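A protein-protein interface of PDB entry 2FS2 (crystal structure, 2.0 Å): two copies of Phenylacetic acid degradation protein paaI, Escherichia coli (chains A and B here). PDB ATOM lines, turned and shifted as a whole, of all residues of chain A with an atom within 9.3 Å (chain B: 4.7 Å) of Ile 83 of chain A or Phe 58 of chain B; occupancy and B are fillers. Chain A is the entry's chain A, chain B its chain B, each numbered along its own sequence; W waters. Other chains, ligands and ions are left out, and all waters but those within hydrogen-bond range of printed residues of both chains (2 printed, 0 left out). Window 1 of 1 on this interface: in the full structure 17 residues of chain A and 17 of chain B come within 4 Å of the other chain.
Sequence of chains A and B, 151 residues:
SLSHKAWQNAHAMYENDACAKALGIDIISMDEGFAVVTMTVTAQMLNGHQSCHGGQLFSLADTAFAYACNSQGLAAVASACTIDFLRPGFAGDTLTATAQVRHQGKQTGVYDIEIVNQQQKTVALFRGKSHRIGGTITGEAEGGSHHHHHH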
ATOM      1  N   CYS A  52     -11.742  -6.036  -7.068  1.00  0.00           N
ATOM      2  CA  CYS A  52     -11.834  -7.359  -6.515  1.00  0.00           C
ATOM      3  C   CYS A  52     -13.161  -8.046  -6.980  1.00  0.00           C
ATOM      4  O   CYS A  52     -14.228  -7.441  -6.942  1.00  0.00           O
ATOM      5  CB  CYS A  52     -11.731  -7.252  -4.998  1.00  0.00           C
ATOM      6  SG  CYS A  52     -11.385  -8.842  -4.364  1.00  0.00           S
ATOM      7  N   HIS A  53     -13.087  -9.245  -7.514  1.00  0.00           N
ATOM      8  CA  HIS A  53     -14.346  -9.910  -7.795  1.00  0.00           C
ATOM      9  C   HIS A  53     -15.187 -10.272  -6.543  1.00  0.00           C
ATOM     10  O   HIS A  53     -14.638 -10.568  -5.463  1.00  0.00           O
ATOM     11  CB  HIS A  53     -14.223 -10.934  -8.894  1.00  0.00           C
ATOM     12  CG  HIS A  53     -13.768 -12.287  -8.473  1.00  0.00           C
ATOM     13  ND1 HIS A  53     -12.446 -12.582  -8.206  1.00  0.00           N
ATOM     14  CD2 HIS A  53     -14.444 -13.471  -8.383  1.00  0.00           C
ATOM     15  CE1 HIS A  53     -12.330 -13.877  -7.911  1.00  0.00           C
ATOM     16  NE2 HIS A  53     -13.528 -14.436  -8.004  1.00  0.00           N
ATOM     17  N   GLY A  54     -16.488 -10.027  -6.634  1.00  0.00           N
ATOM     18  CA  GLY A  54     -17.398 -10.360  -5.580  1.00  0.00           C
ATOM     19  C   GLY A  54     -17.191 -11.733  -4.945  1.00  0.00           C
ATOM     20  O   GLY A  54     -17.417 -11.850  -3.801  1.00  0.00           O
ATOM     21  N   GLY A  55     -16.682 -12.741  -5.636  1.00  0.00           N
ATOM     22  CA  GLY A  55     -16.486 -14.051  -5.050  1.00  0.00           C
ATOM     23  C   GLY A  55     -15.271 -14.179  -4.198  1.00  0.00           C
ATOM     24  O   GLY A  55     -15.168 -15.066  -3.313  1.00  0.00           O
ATOM     25  N   GLN A  56     -14.309 -13.299  -4.421  1.00  0.00           N
ATOM     26  CA  GLN A  56     -13.209 -13.256  -3.479  1.00  0.00           C
ATOM     27  C   GLN A  56     -13.632 -12.506  -2.249  1.00  0.00           C
ATOM     28  O   GLN A  56     -13.308 -12.921  -1.128  1.00  0.00           O
ATOM     29  CB  GLN A  56     -12.000 -12.552  -4.075  1.00  0.00           C
ATOM     30  CG  GLN A  56     -11.066 -13.463  -4.849  1.00  0.00           C
ATOM     31  CD  GLN A  56     -10.319 -14.383  -3.967  1.00  0.00           C
ATOM     32  OE1 GLN A  56      -9.687 -13.942  -2.991  1.00  0.00           O
ATOM     33  NE2 GLN A  56     -10.425 -15.696  -4.248  1.00  0.00           N
ATOM     34  N   LEU A  57     -14.321 -11.378  -2.425  1.00  0.00           N
ATOM     35  CA  LEU A  57     -14.839 -10.726  -1.265  1.00  0.00           C
ATOM     36  C   LEU A  57     -15.699 -11.741  -0.468  1.00  0.00           C
ATOM     37  O   LEU A  57     -15.683 -11.720   0.721  1.00  0.00           O
ATOM     38  CB  LEU A  57     -15.715  -9.538  -1.622  1.00  0.00           C
ATOM     39  CG  LEU A  57     -14.931  -8.309  -2.164  1.00  0.00           C
ATOM     40  CD1 LEU A  57     -15.894  -7.151  -2.665  1.00  0.00           C
ATOM     41  CD2 LEU A  57     -13.999  -7.751  -1.058  1.00  0.00           C
ATOM     42  N   PHE A  58     -16.487 -12.566  -1.140  1.00  0.00           N
ATOM     43  CA  PHE A  58     -17.427 -13.450  -0.419  1.00  0.00           C
ATOM     44  C   PHE A  58     -16.596 -14.475   0.362  1.00  0.00           C
ATOM     45  O   PHE A  58     -16.880 -14.742   1.567  1.00  0.00           O
ATOM     46  CB  PHE A  58     -18.464 -14.050  -1.370  1.00  0.00           C
ATOM     47  CG  PHE A  58     -19.289 -15.063  -0.753  1.00  0.00           C
ATOM     48  CD1 PHE A  58     -20.591 -14.785  -0.423  1.00  0.00           C
ATOM     49  CD2 PHE A  58     -18.745 -16.309  -0.406  1.00  0.00           C
ATOM     50  CE1 PHE A  58     -21.322 -15.706   0.255  1.00  0.00           C
ATOM     51  CE2 PHE A  58     -19.512 -17.229   0.222  1.00  0.00           C
ATOM     52  CZ  PHE A  58     -20.807 -16.914   0.572  1.00  0.00           C
ATOM     53  N   SER A  59     -15.496 -14.938  -0.215  1.00  0.00           N
ATOM     54  CA  SER A  59     -14.620 -15.871   0.501  1.00  0.00           C
ATOM     55  C   SER A  59     -13.877 -15.339   1.651  1.00  0.00           C
ATOM     56  O   SER A  59     -13.583 -16.049   2.647  1.00  0.00           O
ATOM     57  CB  SER A  59     -13.579 -16.555  -0.432  1.00  0.00           C
ATOM     58  OG  SER A  59     -14.268 -17.265  -1.411  1.00  0.00           O
ATOM     59  N   ALA A  61     -14.935 -12.832   3.483  1.00  0.00           N
ATOM     60  CA  ALA A  61     -15.994 -12.798   4.519  1.00  0.00           C
ATOM     61  C   ALA A  61     -16.376 -14.222   5.080  1.00  0.00           C
ATOM     62  O   ALA A  61     -16.507 -14.368   6.261  1.00  0.00           O
ATOM     63  CB  ALA A  61     -17.199 -12.160   3.942  1.00  0.00           C
ATOM     64  N   ASP A  62     -16.617 -15.222   4.240  1.00  0.00           N
ATOM     65  CA  ASP A  62     -16.802 -16.634   4.670  1.00  0.00           C
ATOM     66  C   ASP A  62     -15.696 -17.190   5.600  1.00  0.00           C
ATOM     67  O   ASP A  62     -15.951 -17.887   6.584  1.00  0.00           O
ATOM     68  CB  ASP A  62     -16.963 -17.537   3.465  1.00  0.00           C
ATOM     69  CG  ASP A  62     -17.472 -18.956   3.816  1.00  0.00           C
ATOM     70  OD1 ASP A  62     -16.786 -19.931   3.381  1.00  0.00           O
ATOM     71  OD2 ASP A  62     -18.525 -19.229   4.530  1.00  0.00           O
ATOM     72  N   ALA A  80     -27.781 -18.609   4.361  1.00  0.00           N
ATOM     73  CA  ALA A  80     -28.270 -17.476   3.587  1.00  0.00           C
ATOM     74  C   ALA A  80     -27.248 -16.397   3.848  1.00  0.00           C
ATOM     75  O   ALA A  80     -26.552 -16.427   4.862  1.00  0.00           O
ATOM     76  CB  ALA A  80     -29.652 -16.995   4.058  1.00  0.00           C
ATOM     77  N   CYS A  81     -27.127 -15.435   2.932  1.00  0.00           N
ATOM     78  CA  CYS A  81     -26.206 -14.300   3.160  1.00  0.00           C
ATOM     79  C   CYS A  81     -26.730 -13.086   2.430  1.00  0.00           C
ATOM     80  O   CYS A  81     -27.287 -13.218   1.367  1.00  0.00           O
ATOM     81  CB  CYS A  81     -24.826 -14.605   2.662  1.00  0.00           C
ATOM     82  SG  CYS A  81     -23.815 -13.241   3.291  1.00  0.00           S
ATOM     83  N   THR A  82     -26.661 -11.936   3.041  1.00  0.00           N
ATOM     84  CA  THR A  82     -27.021 -10.650   2.351  1.00  0.00           C
ATOM     85  C   THR A  82     -25.777  -9.797   2.345  1.00  0.00           C
ATOM     86  O   THR A  82     -25.034  -9.848   3.289  1.00  0.00           O
ATOM     87  CB  THR A  82     -28.167  -9.927   3.102  1.00  0.00           C
ATOM     88  OG1 THR A  82     -29.367 -10.686   2.903  1.00  0.00           O
ATOM     89  CG2 THR A  82     -28.565  -8.560   2.358  1.00  0.00           C
ATOM     90  N   ILE A  83     -25.505  -9.077   1.249  1.00  0.00           N
ATOM     91  CA  ILE A  83     -24.224  -8.327   1.034  1.00  0.00           C
ATOM     92  C   ILE A  83     -24.566  -7.005   0.393  1.00  0.00           C
ATOM     93  O   ILE A  83     -25.349  -7.027  -0.485  1.00  0.00           O
ATOM     94  CB  ILE A  83     -23.349  -9.022   0.045  1.00  0.00           C
ATOM     95  CG1 ILE A  83     -23.298 -10.506   0.344  1.00  0.00           C
ATOM     96  CG2 ILE A  83     -22.020  -8.430   0.118  1.00  0.00           C
ATOM     97  CD1 ILE A  83     -22.518 -11.217  -0.793  1.00  0.00           C
ATOM     98  N   ASP A  84     -24.115  -5.896   0.993  1.00  0.00           N
ATOM     99  CA  ASP A  84     -24.078  -4.575   0.338  1.00  0.00           C
ATOM    100  C   ASP A  84     -22.656  -4.272  -0.100  1.00  0.00           C
ATOM    101  O   ASP A  84     -21.749  -4.300   0.732  1.00  0.00           O
ATOM    102  CB  ASP A  84     -24.554  -3.547   1.326  1.00  0.00           C
ATOM    103  CG  ASP A  84     -26.052  -3.762   1.685  1.00  0.00           C
ATOM    104  OD1 ASP A  84     -26.952  -3.281   0.900  1.00  0.00           O
ATOM    105  OD2 ASP A  84     -26.463  -4.438   2.693  1.00  0.00           O
ATOM    106  N   PHE A  85     -22.424  -3.957  -1.378  1.00  0.00           N
ATOM    107  CA  PHE A  85     -21.039  -3.605  -1.827  1.00  0.00           C
ATOM    108  C   PHE A  85     -21.008  -2.068  -1.822  1.00  0.00           C
ATOM    109  O   PHE A  85     -21.880  -1.470  -2.465  1.00  0.00           O
ATOM    110  CB  PHE A  85     -20.916  -4.055  -3.237  1.00  0.00           C
ATOM    111  CG  PHE A  85     -21.013  -5.510  -3.388  1.00  0.00           C
ATOM    112  CD1 PHE A  85     -22.175  -6.062  -3.858  1.00  0.00           C
ATOM    113  CD2 PHE A  85     -19.918  -6.359  -3.040  1.00  0.00           C
ATOM    114  CE1 PHE A  85     -22.353  -7.446  -3.991  1.00  0.00           C
ATOM    115  CE2 PHE A  85     -20.028  -7.815  -3.230  1.00  0.00           C
ATOM    116  CZ  PHE A  85     -21.253  -8.349  -3.717  1.00  0.00           C
ATOM    117  N   LEU A  86     -20.143  -1.404  -1.052  1.00  0.00           N
ATOM    118  CA  LEU A  86     -20.208   0.075  -0.991  1.00  0.00           C
ATOM    119  C   LEU A  86     -19.146   0.766  -1.851  1.00  0.00           C
ATOM    120  O   LEU A  86     -19.386   1.875  -2.309  1.00  0.00           O
ATOM    121  CB  LEU A  86     -20.071   0.593   0.466  1.00  0.00           C
ATOM    122  CG  LEU A  86     -21.002  -0.149   1.453  1.00  0.00           C
ATOM    123  CD1 LEU A  86     -21.102   0.555   2.745  1.00  0.00           C
ATOM    124  CD2 LEU A  86     -22.383  -0.119   0.927  1.00  0.00           C
ATOM    125  N   ILE A 113     -20.569  -9.364   9.067  1.00  0.00           N
ATOM    126  CA  ILE A 113     -19.180  -9.183   8.699  1.00  0.00           C
ATOM    127  C   ILE A 113     -19.052  -7.824   8.007  1.00  0.00           C
ATOM    128  O   ILE A 113     -19.863  -7.493   7.211  1.00  0.00           O
ATOM    129  CB  ILE A 113     -18.795 -10.240   7.715  1.00  0.00           C
ATOM    130  CG1 ILE A 113     -18.838 -11.596   8.390  1.00  0.00           C
ATOM    131  CG2 ILE A 113     -17.286 -10.092   7.301  1.00  0.00           C
ATOM    132  CD1 ILE A 113     -20.032 -12.456   7.970  1.00  0.00           C
ATOM    133  N   GLU A 114     -18.060  -7.032   8.371  1.00  0.00           N
ATOM    134  CA  GLU A 114     -17.795  -5.764   7.679  1.00  0.00           C
ATOM    135  C   GLU A 114     -16.390  -5.931   7.032  1.00  0.00           C
ATOM    136  O   GLU A 114     -15.496  -6.435   7.695  1.00  0.00           O
ATOM    137  CB  GLU A 114     -17.740  -4.663   8.739  1.00  0.00           C
ATOM    138  CG  GLU A 114     -17.445  -3.286   8.086  1.00  0.00           C
ATOM    139  CD  GLU A 114     -17.792  -2.086   8.962  1.00  0.00           C
ATOM    140  OE1 GLU A 114     -17.994  -2.265  10.180  1.00  0.00           O
ATOM    141  OE2 GLU A 114     -17.841  -0.915   8.459  1.00  0.00           O
ATOM    142  N   ILE A 115     -16.219  -5.565   5.771  1.00  0.00           N
ATOM    143  CA  ILE A 115     -14.901  -5.503   5.170  1.00  0.00           C
ATOM    144  C   ILE A 115     -14.599  -4.007   4.998  1.00  0.00           C
ATOM    145  O   ILE A 115     -15.436  -3.277   4.530  1.00  0.00           O
ATOM    146  CB  ILE A 115     -14.925  -6.159   3.827  1.00  0.00           C
ATOM    147  CG1 ILE A 115     -15.317  -7.628   3.993  1.00  0.00           C
ATOM    148  CG2 ILE A 115     -13.484  -6.036   3.067  1.00  0.00           C
ATOM    149  CD1 ILE A 115     -15.325  -8.406   2.706  1.00  0.00           C
ATOM    150  N   VAL A 123     -15.925  -1.339   2.547  1.00  0.00           N
ATOM    151  CA  VAL A 123     -15.979  -1.869   1.216  1.00  0.00           C
ATOM    152  C   VAL A 123     -17.250  -2.674   1.063  1.00  0.00           C
ATOM    153  O   VAL A 123     -17.939  -2.565   0.049  1.00  0.00           O
ATOM    154  CB  VAL A 123     -14.676  -2.711   0.986  1.00  0.00           C
ATOM    155  CG1 VAL A 123     -14.854  -3.733  -0.158  1.00  0.00           C
ATOM    156  CG2 VAL A 123     -13.477  -1.783   0.733  1.00  0.00           C
ATOM    157  N   ALA A 124     -17.590  -3.529   2.054  1.00  0.00           N
ATOM    158  CA  ALA A 124     -18.778  -4.337   1.929  1.00  0.00           C
ATOM    159  C   ALA A 124     -19.351  -4.650   3.335  1.00  0.00           C
ATOM    160  O   ALA A 124     -18.610  -4.688   4.232  1.00  0.00           O
ATOM    161  CB  ALA A 124     -18.413  -5.628   1.234  1.00  0.00           C
ATOM    162  N   LEU A 125     -20.650  -4.797   3.492  1.00  0.00           N
ATOM    163  CA  LEU A 125     -21.334  -5.402   4.669  1.00  0.00           C
ATOM    164  C   LEU A 125     -22.030  -6.735   4.373  1.00  0.00           C
ATOM    165  O   LEU A 125     -22.708  -6.837   3.336  1.00  0.00           O
ATOM    166  CB  LEU A 125     -22.362  -4.415   5.193  1.00  0.00           C
ATOM    167  CG  LEU A 125     -21.807  -3.025   5.518  1.00  0.00           C
ATOM    168  CD1 LEU A 125     -22.967  -1.974   5.751  1.00  0.00           C
ATOM    169  CD2 LEU A 125     -21.001  -3.210   6.788  1.00  0.00           C
ATOM    170  N   PHE A 126     -21.827  -7.770   5.227  1.00  0.00           N
ATOM    171  CA  PHE A 126     -22.530  -9.014   5.069  1.00  0.00           C
ATOM    172  C   PHE A 126     -23.343  -9.207   6.346  1.00  0.00           C
ATOM    173  O   PHE A 126     -22.862  -8.966   7.422  1.00  0.00           O
ATOM    174  CB  PHE A 126     -21.548 -10.205   5.014  1.00  0.00           C
ATOM    175  CG  PHE A 126     -20.606 -10.153   3.858  1.00  0.00           C
ATOM    176  CD1 PHE A 126     -19.603  -9.144   3.784  1.00  0.00           C
ATOM    177  CD2 PHE A 126     -20.725 -11.095   2.851  1.00  0.00           C
ATOM    178  CE1 PHE A 126     -18.744  -9.016   2.663  1.00  0.00           C
ATOM    179  CE2 PHE A 126     -19.811 -11.060   1.663  1.00  0.00           C
ATOM    180  CZ  PHE A 126     -18.819 -10.014   1.589  1.00  0.00           C
ATOM    181  N   ARG A 127     -24.497  -9.769   6.204  1.00  0.00           N
ATOM    182  CA  ARG A 127     -25.114 -10.450   7.317  1.00  0.00           C
ATOM    183  C   ARG A 127     -25.435 -11.883   6.889  1.00  0.00           C
ATOM    184  O   ARG A 127     -26.099 -12.092   5.898  1.00  0.00           O
ATOM    185  CB  ARG A 127     -26.416  -9.713   7.653  1.00  0.00           C
ATOM    186  CG  ARG A 127     -27.227 -10.410   8.913  1.00  0.00           C
ATOM    187  CD  ARG A 127     -28.146  -9.309   9.786  1.00  0.00           C
ATOM    188  NE  ARG A 127     -27.432  -8.193  10.456  1.00  0.00           N
ATOM    189  CZ  ARG A 127     -28.029  -7.018  10.833  1.00  0.00           C
ATOM    190  NH1 ARG A 127     -29.337  -6.845  10.568  1.00  0.00           N
ATOM    191  NH2 ARG A 127     -27.332  -6.038  11.453  1.00  0.00           N
ATOM    192  N   GLY A 128     -24.957 -12.869   7.641  1.00  0.00           N
ATOM    193  CA  GLY A 128     -25.170 -14.265   7.359  1.00  0.00           C
ATOM    194  C   GLY A 128     -26.013 -15.006   8.388  1.00  0.00           C
ATOM    195  O   GLY A 128     -25.927 -14.705   9.563  1.00  0.00           O
ATOM    196  N   GLY B  54     -19.048 -22.053  -0.896  1.00  0.00           N
ATOM    197  CA  GLY B  54     -19.945 -20.935  -1.131  1.00  0.00           C
ATOM    198  C   GLY B  54     -19.399 -19.912  -2.136  1.00  0.00           C
ATOM    199  O   GLY B  54     -20.108 -19.478  -3.005  1.00  0.00           O
ATOM    200  N   GLY B  55     -18.158 -19.522  -1.986  1.00  0.00           N
ATOM    201  CA  GLY B  55     -17.596 -18.550  -2.876  1.00  0.00           C
ATOM    202  C   GLY B  55     -17.619 -18.965  -4.319  1.00  0.00           C
ATOM    203  O   GLY B  55     -17.731 -18.087  -5.166  1.00  0.00           O
ATOM    204  N   GLN B  56     -17.527 -20.273  -4.591  1.00  0.00           N
ATOM    205  CA  GLN B  56     -17.597 -20.778  -5.979  1.00  0.00           C
ATOM    206  C   GLN B  56     -19.033 -20.739  -6.466  1.00  0.00           C
ATOM    207  O   GLN B  56     -19.266 -20.473  -7.630  1.00  0.00           O
ATOM    208  CB  GLN B  56     -17.070 -22.231  -6.105  1.00  0.00           C
ATOM    209  CG  GLN B  56     -15.507 -22.394  -6.351  1.00  0.00           C
ATOM    210  CD  GLN B  56     -14.656 -22.521  -5.021  1.00  0.00           C
ATOM    211  OE1 GLN B  56     -15.092 -22.054  -3.956  1.00  0.00           O
ATOM    212  NE2 GLN B  56     -13.430 -23.123  -5.115  1.00  0.00           N
ATOM    213  N   LEU B  57     -19.965 -21.110  -5.583  1.00  0.00           N
ATOM    214  CA  LEU B  57     -21.359 -21.002  -5.866  1.00  0.00           C
ATOM    215  C   LEU B  57     -21.732 -19.547  -6.026  1.00  0.00           C
ATOM    216  O   LEU B  57     -22.353 -19.226  -7.022  1.00  0.00           O
ATOM    217  CB  LEU B  57     -22.167 -21.530  -4.724  1.00  0.00           C
ATOM    218  CG  LEU B  57     -22.423 -23.006  -4.684  1.00  0.00           C
ATOM    219  CD1 LEU B  57     -23.618 -23.268  -3.758  1.00  0.00           C
ATOM    220  CD2 LEU B  57     -22.651 -23.521  -6.123  1.00  0.00           C
ATOM    221  N   PHE B  58     -21.330 -18.672  -5.079  1.00  0.00           N
ATOM    222  CA  PHE B  58     -21.572 -17.243  -5.213  1.00  0.00           C
ATOM    223  C   PHE B  58     -21.010 -16.788  -6.578  1.00  0.00           C
ATOM    224  O   PHE B  58     -21.630 -16.040  -7.291  1.00  0.00           O
ATOM    225  CB  PHE B  58     -20.941 -16.432  -4.052  1.00  0.00           C
ATOM    226  CG  PHE B  58     -21.087 -14.925  -4.218  1.00  0.00           C
ATOM    227  CD1 PHE B  58     -22.168 -14.272  -3.730  1.00  0.00           C
ATOM    228  CD2 PHE B  58     -20.180 -14.189  -4.944  1.00  0.00           C
ATOM    229  CE1 PHE B  58     -22.341 -12.892  -3.963  1.00  0.00           C
ATOM    230  CE2 PHE B  58     -20.345 -12.817  -5.171  1.00  0.00           C
ATOM    231  CZ  PHE B  58     -21.405 -12.181  -4.670  1.00  0.00           C
ATOM    232  N   SER B  59     -19.870 -17.293  -6.981  1.00  0.00           N
ATOM    233  CA  SER B  59     -19.228 -16.795  -8.208  1.00  0.00           C
ATOM    234  C   SER B  59     -19.954 -17.197  -9.449  1.00  0.00           C
ATOM    235  O   SER B  59     -20.022 -16.398 -10.438  1.00  0.00           O
ATOM    236  CB  SER B  59     -17.811 -17.295  -8.349  1.00  0.00           C
ATOM    237  OG  SER B  59     -17.066 -16.776  -7.278  1.00  0.00           O
ATOM    238  N   LEU B  60     -20.561 -18.378  -9.395  1.00  0.00           N
ATOM    239  CA  LEU B  60     -21.342 -18.793 -10.468  1.00  0.00           C
ATOM    240  C   LEU B  60     -22.595 -17.926 -10.604  1.00  0.00           C
ATOM    241  O   LEU B  60     -23.034 -17.632 -11.713  1.00  0.00           O
ATOM    242  CB  LEU B  60     -21.738 -20.274 -10.258  1.00  0.00           C
ATOM    243  CG  LEU B  60     -22.723 -20.914 -11.253  1.00  0.00           C
ATOM    244  CD1 LEU B  60     -22.148 -20.900 -12.712  1.00  0.00           C
ATOM    245  CD2 LEU B  60     -22.991 -22.388 -10.843  1.00  0.00           C
ATOM    246  N   ALA B  61     -23.241 -17.605  -9.461  1.00  0.00           N
ATOM    247  CA  ALA B  61     -24.472 -16.837  -9.516  1.00  0.00           C
ATOM    248  C   ALA B  61     -24.167 -15.402 -10.027  1.00  0.00           C
ATOM    249  O   ALA B  61     -24.923 -14.836 -10.800  1.00  0.00           O
ATOM    250  CB  ALA B  61     -25.184 -16.808  -8.095  1.00  0.00           C
ATOM    251  N   ASP B  62     -23.027 -14.895  -9.675  1.00  0.00           N
ATOM    252  CA  ASP B  62     -22.630 -13.520  -9.884  1.00  0.00           C
ATOM    253  C   ASP B  62     -22.217 -13.420 -11.309  1.00  0.00           C
ATOM    254  O   ASP B  62     -22.339 -12.367 -11.924  1.00  0.00           O
ATOM    255  CB  ASP B  62     -21.409 -13.250  -8.984  1.00  0.00           C
ATOM    256  CG  ASP B  62     -20.935 -11.780  -9.006  1.00  0.00           C
ATOM    257  OD1 ASP B  62     -21.776 -10.829  -9.183  1.00  0.00           O
ATOM    258  OD2 ASP B  62     -19.737 -11.466  -8.801  1.00  0.00           O
ATOM    259  N   SER B  79     -24.789  -3.693  -6.681  1.00  0.00           N
ATOM    260  CA  SER B  79     -24.639  -2.950  -5.437  1.00  0.00           C
ATOM    261  C   SER B  79     -25.005  -3.790  -4.219  1.00  0.00           C
ATOM    262  O   SER B  79     -24.667  -3.421  -3.082  1.00  0.00           O
ATOM    263  CB  SER B  79     -25.545  -1.741  -5.357  1.00  0.00           C
ATOM    264  OG  SER B  79     -26.746  -2.135  -5.790  1.00  0.00           O
ATOM    265  N   ALA B  80     -25.742  -4.866  -4.410  1.00  0.00           N
ATOM    266  CA  ALA B  80     -26.187  -5.659  -3.259  1.00  0.00           C
ATOM    267  C   ALA B  80     -26.760  -6.943  -3.751  1.00  0.00           C
ATOM    268  O   ALA B  80     -27.171  -7.085  -4.916  1.00  0.00           O
ATOM    269  CB  ALA B  80     -27.302  -4.927  -2.428  1.00  0.00           C
ATOM    270  N   CYS B  81     -26.832  -7.915  -2.834  1.00  0.00           N
ATOM    271  CA  CYS B  81     -27.451  -9.140  -3.225  1.00  0.00           C
ATOM    272  C   CYS B  81     -27.616 -10.111  -2.077  1.00  0.00           C
ATOM    273  O   CYS B  81     -26.961  -9.952  -1.095  1.00  0.00           O
ATOM    274  CB  CYS B  81     -26.589  -9.753  -4.272  1.00  0.00           C
ATOM    275  SG  CYS B  81     -25.165 -10.477  -3.608  1.00  0.00           S
ATOM    276  N   ILE B  83     -28.158 -14.408  -1.052  1.00  0.00           N
ATOM    277  CA  ILE B  83     -28.079 -15.776  -1.517  1.00  0.00           C
ATOM    278  C   ILE B  83     -28.688 -16.696  -0.447  1.00  0.00           C
ATOM    279  O   ILE B  83     -28.414 -16.497   0.689  1.00  0.00           O
ATOM    280  CB  ILE B  83     -26.561 -16.169  -2.040  1.00  0.00           C
ATOM    281  CG1 ILE B  83     -26.417 -17.633  -2.394  1.00  0.00           C
ATOM    282  CG2 ILE B  83     -25.420 -15.889  -1.024  1.00  0.00           C
ATOM    283  CD1 ILE B  83     -25.410 -17.936  -3.717  1.00  0.00           C
ATOM    284  N   PHE B 126     -30.677 -16.547  -5.621  1.00  0.00           N
ATOM    285  CA  PHE B 126     -29.888 -15.392  -5.350  1.00  0.00           C
ATOM    286  C   PHE B 126     -30.753 -14.281  -5.962  1.00  0.00           C
ATOM    287  O   PHE B 126     -31.529 -14.530  -6.871  1.00  0.00           O
ATOM    288  CB  PHE B 126     -28.635 -15.630  -6.132  1.00  0.00           C
ATOM    289  CG  PHE B 126     -27.804 -14.449  -6.372  1.00  0.00           C
ATOM    290  CD1 PHE B 126     -26.512 -14.375  -5.779  1.00  0.00           C
ATOM    291  CD2 PHE B 126     -28.210 -13.458  -7.233  1.00  0.00           C
ATOM    292  CE1 PHE B 126     -25.670 -13.264  -6.019  1.00  0.00           C
ATOM    293  CE2 PHE B 126     -27.360 -12.307  -7.513  1.00  0.00           C
ATOM    294  CZ  PHE B 126     -26.106 -12.221  -6.918  1.00  0.00           C
HETATM  295  O   HOH W   1     -16.059 -19.756   0.433  1.00  0.00           O
HETATM  296  O   HOH W   2     -26.225  -1.440  -0.970  1.00  0.00           O
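The backbone NH (N) of Ile 83 of chain A sits at hydrogen-bond distance from the backbone carbonyl oxygen (O) of Cys 81 of chain B.
The backbone NH of Cys 81 of chain A lies within hydrogen-bond range of the backbone carbonyl oxygen of Ile 83 of chain B, at 2.8 Å.
The backbone carbonyl oxygen of Ser 79 of chain B sits at hydrogen-bond distance from the backbone NH of Phe 85 of chain A, at 2.9 Å.
Among the printed residues, merely in contact across the chains: Gly 54 of chain A with Phe 58 of chain B, Gly 55 of chain A with Phe 58 of chain B, Gly 55 of chain A with Ser 59 of chain B, Phe 58 of chain A with Gly 54 of chain B, Phe 58 of chain A with Gly 55 of chain B, Phe 58 of chain A with Phe 58 of chain B, Ser 59 of chain A with Gly 55 of chain B, Ala 80 of chain A with Ile 83 of chain B, Thr 82 of chain A with Cys 81 of chain B, Ile 83 of chain A with Phe 58 of chain B, Ile 83 of chain A with Ala 80 of chain B, Asp 84 of chain A with Ser 79 of chain B, Asp 84 of chain A with Ala 80 of chain B, Phe 85 of chain A with Phe 58 of chain B and Phe 85 of chain A with Ala 80 of chain B.
Water W2 lies within hydrogen-bond range of OD1 of Asp 84 of chain A (2.7 Å) and O of Ser 79 of chain B (3.3 Å).
Water W1 bridges OD1 of Asp 62 of chain A and N of Gly 55 of chain B.
Hydrophobic or aromatic side chains of chain A that line the printed part of chain B: Phe 58, Ala 80, Ile 83 and Phe 85.
O of Gly 55 of chain A is in hydrogen-bond range of OG of Ser 59 of chain A (3.0 Å).
SG of Cys 81 of chain A sits close to O of Arg 127 of chain A (3.7 Å).
The backbone NH (N) of Thr 82 of chain A is in hydrogen-bond range of the backbone carbonyl oxygen (O) of Arg 127 of chain A, at 2.9 Å.
N of Asp 84 of chain A sits at hydrogen-bond distance from O of Leu 125 of chain A, at 2.9 Å.
The backbone carbonyl oxygen of Gly 55 of chain B sits at hydrogen-bond distance from the side-chain hydroxyl of Ser 59 of chain B, 2.6 Å away.
Ile 83 of chain A touches three residues of chain B.
Phe 58 of chain B touches just these residues of chain A: Gly 54, Gly 55, Phe 58, Ile 83 and Phe 85.
Gly 55 of chain B touches just these residues of chain A: Phe 58 and Ser 59.
No residue of chain A comes within 4 Å of Ala 61 of chain B.
Cys 81 of chain B touches just these residues of chain A: Thr 82 and Ile 83.
Printed residues of chain B within 4 Å of Thr 82 of chain A: Cys 81 (3.5 Å).
Of the printed residues of chain B, Gly 55 of chain A touches Phe 58 (3.7 Å) and Ser 59 (3.6 Å).
Printed residues of chain A within 4 Å of Ser 79 of chain B: Asp 84 and Phe 85.
Of the printed residues of chain B, Phe 58 of chain A touches Gly 54 (3.6 Å), Gly 55 (3.5 Å) and Phe 58 (3.7 Å).
His 53 of chain A touches none of the printed residues of chain B.
The nearest residue of chain A that does not touch Phe 58 of chain B is His 53 of chain A (5.9 Å).
Gly 55 of chain A touches Phe 58 of chain B, and with the chains exchanged Phe 58 of chain A touches Gly 55 of chain B.
Gly 55 of chain A touches Ser 59 of chain B, and with the chains exchanged Ser 59 of chain A touches Gly 55 of chain B.
Phe 58 of chain B touches its own counterpart, Phe 58 of chain A.
Ile 83 of chain A touches Phe 58 of chain B, but with the chains exchanged Phe 58 of chain A does not touch Ile 83 of chain B (4.3 Å).
Of the 18 pairs that touch across the chains among the printed residues, 11 have their exchanged pair printed and touching as well.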
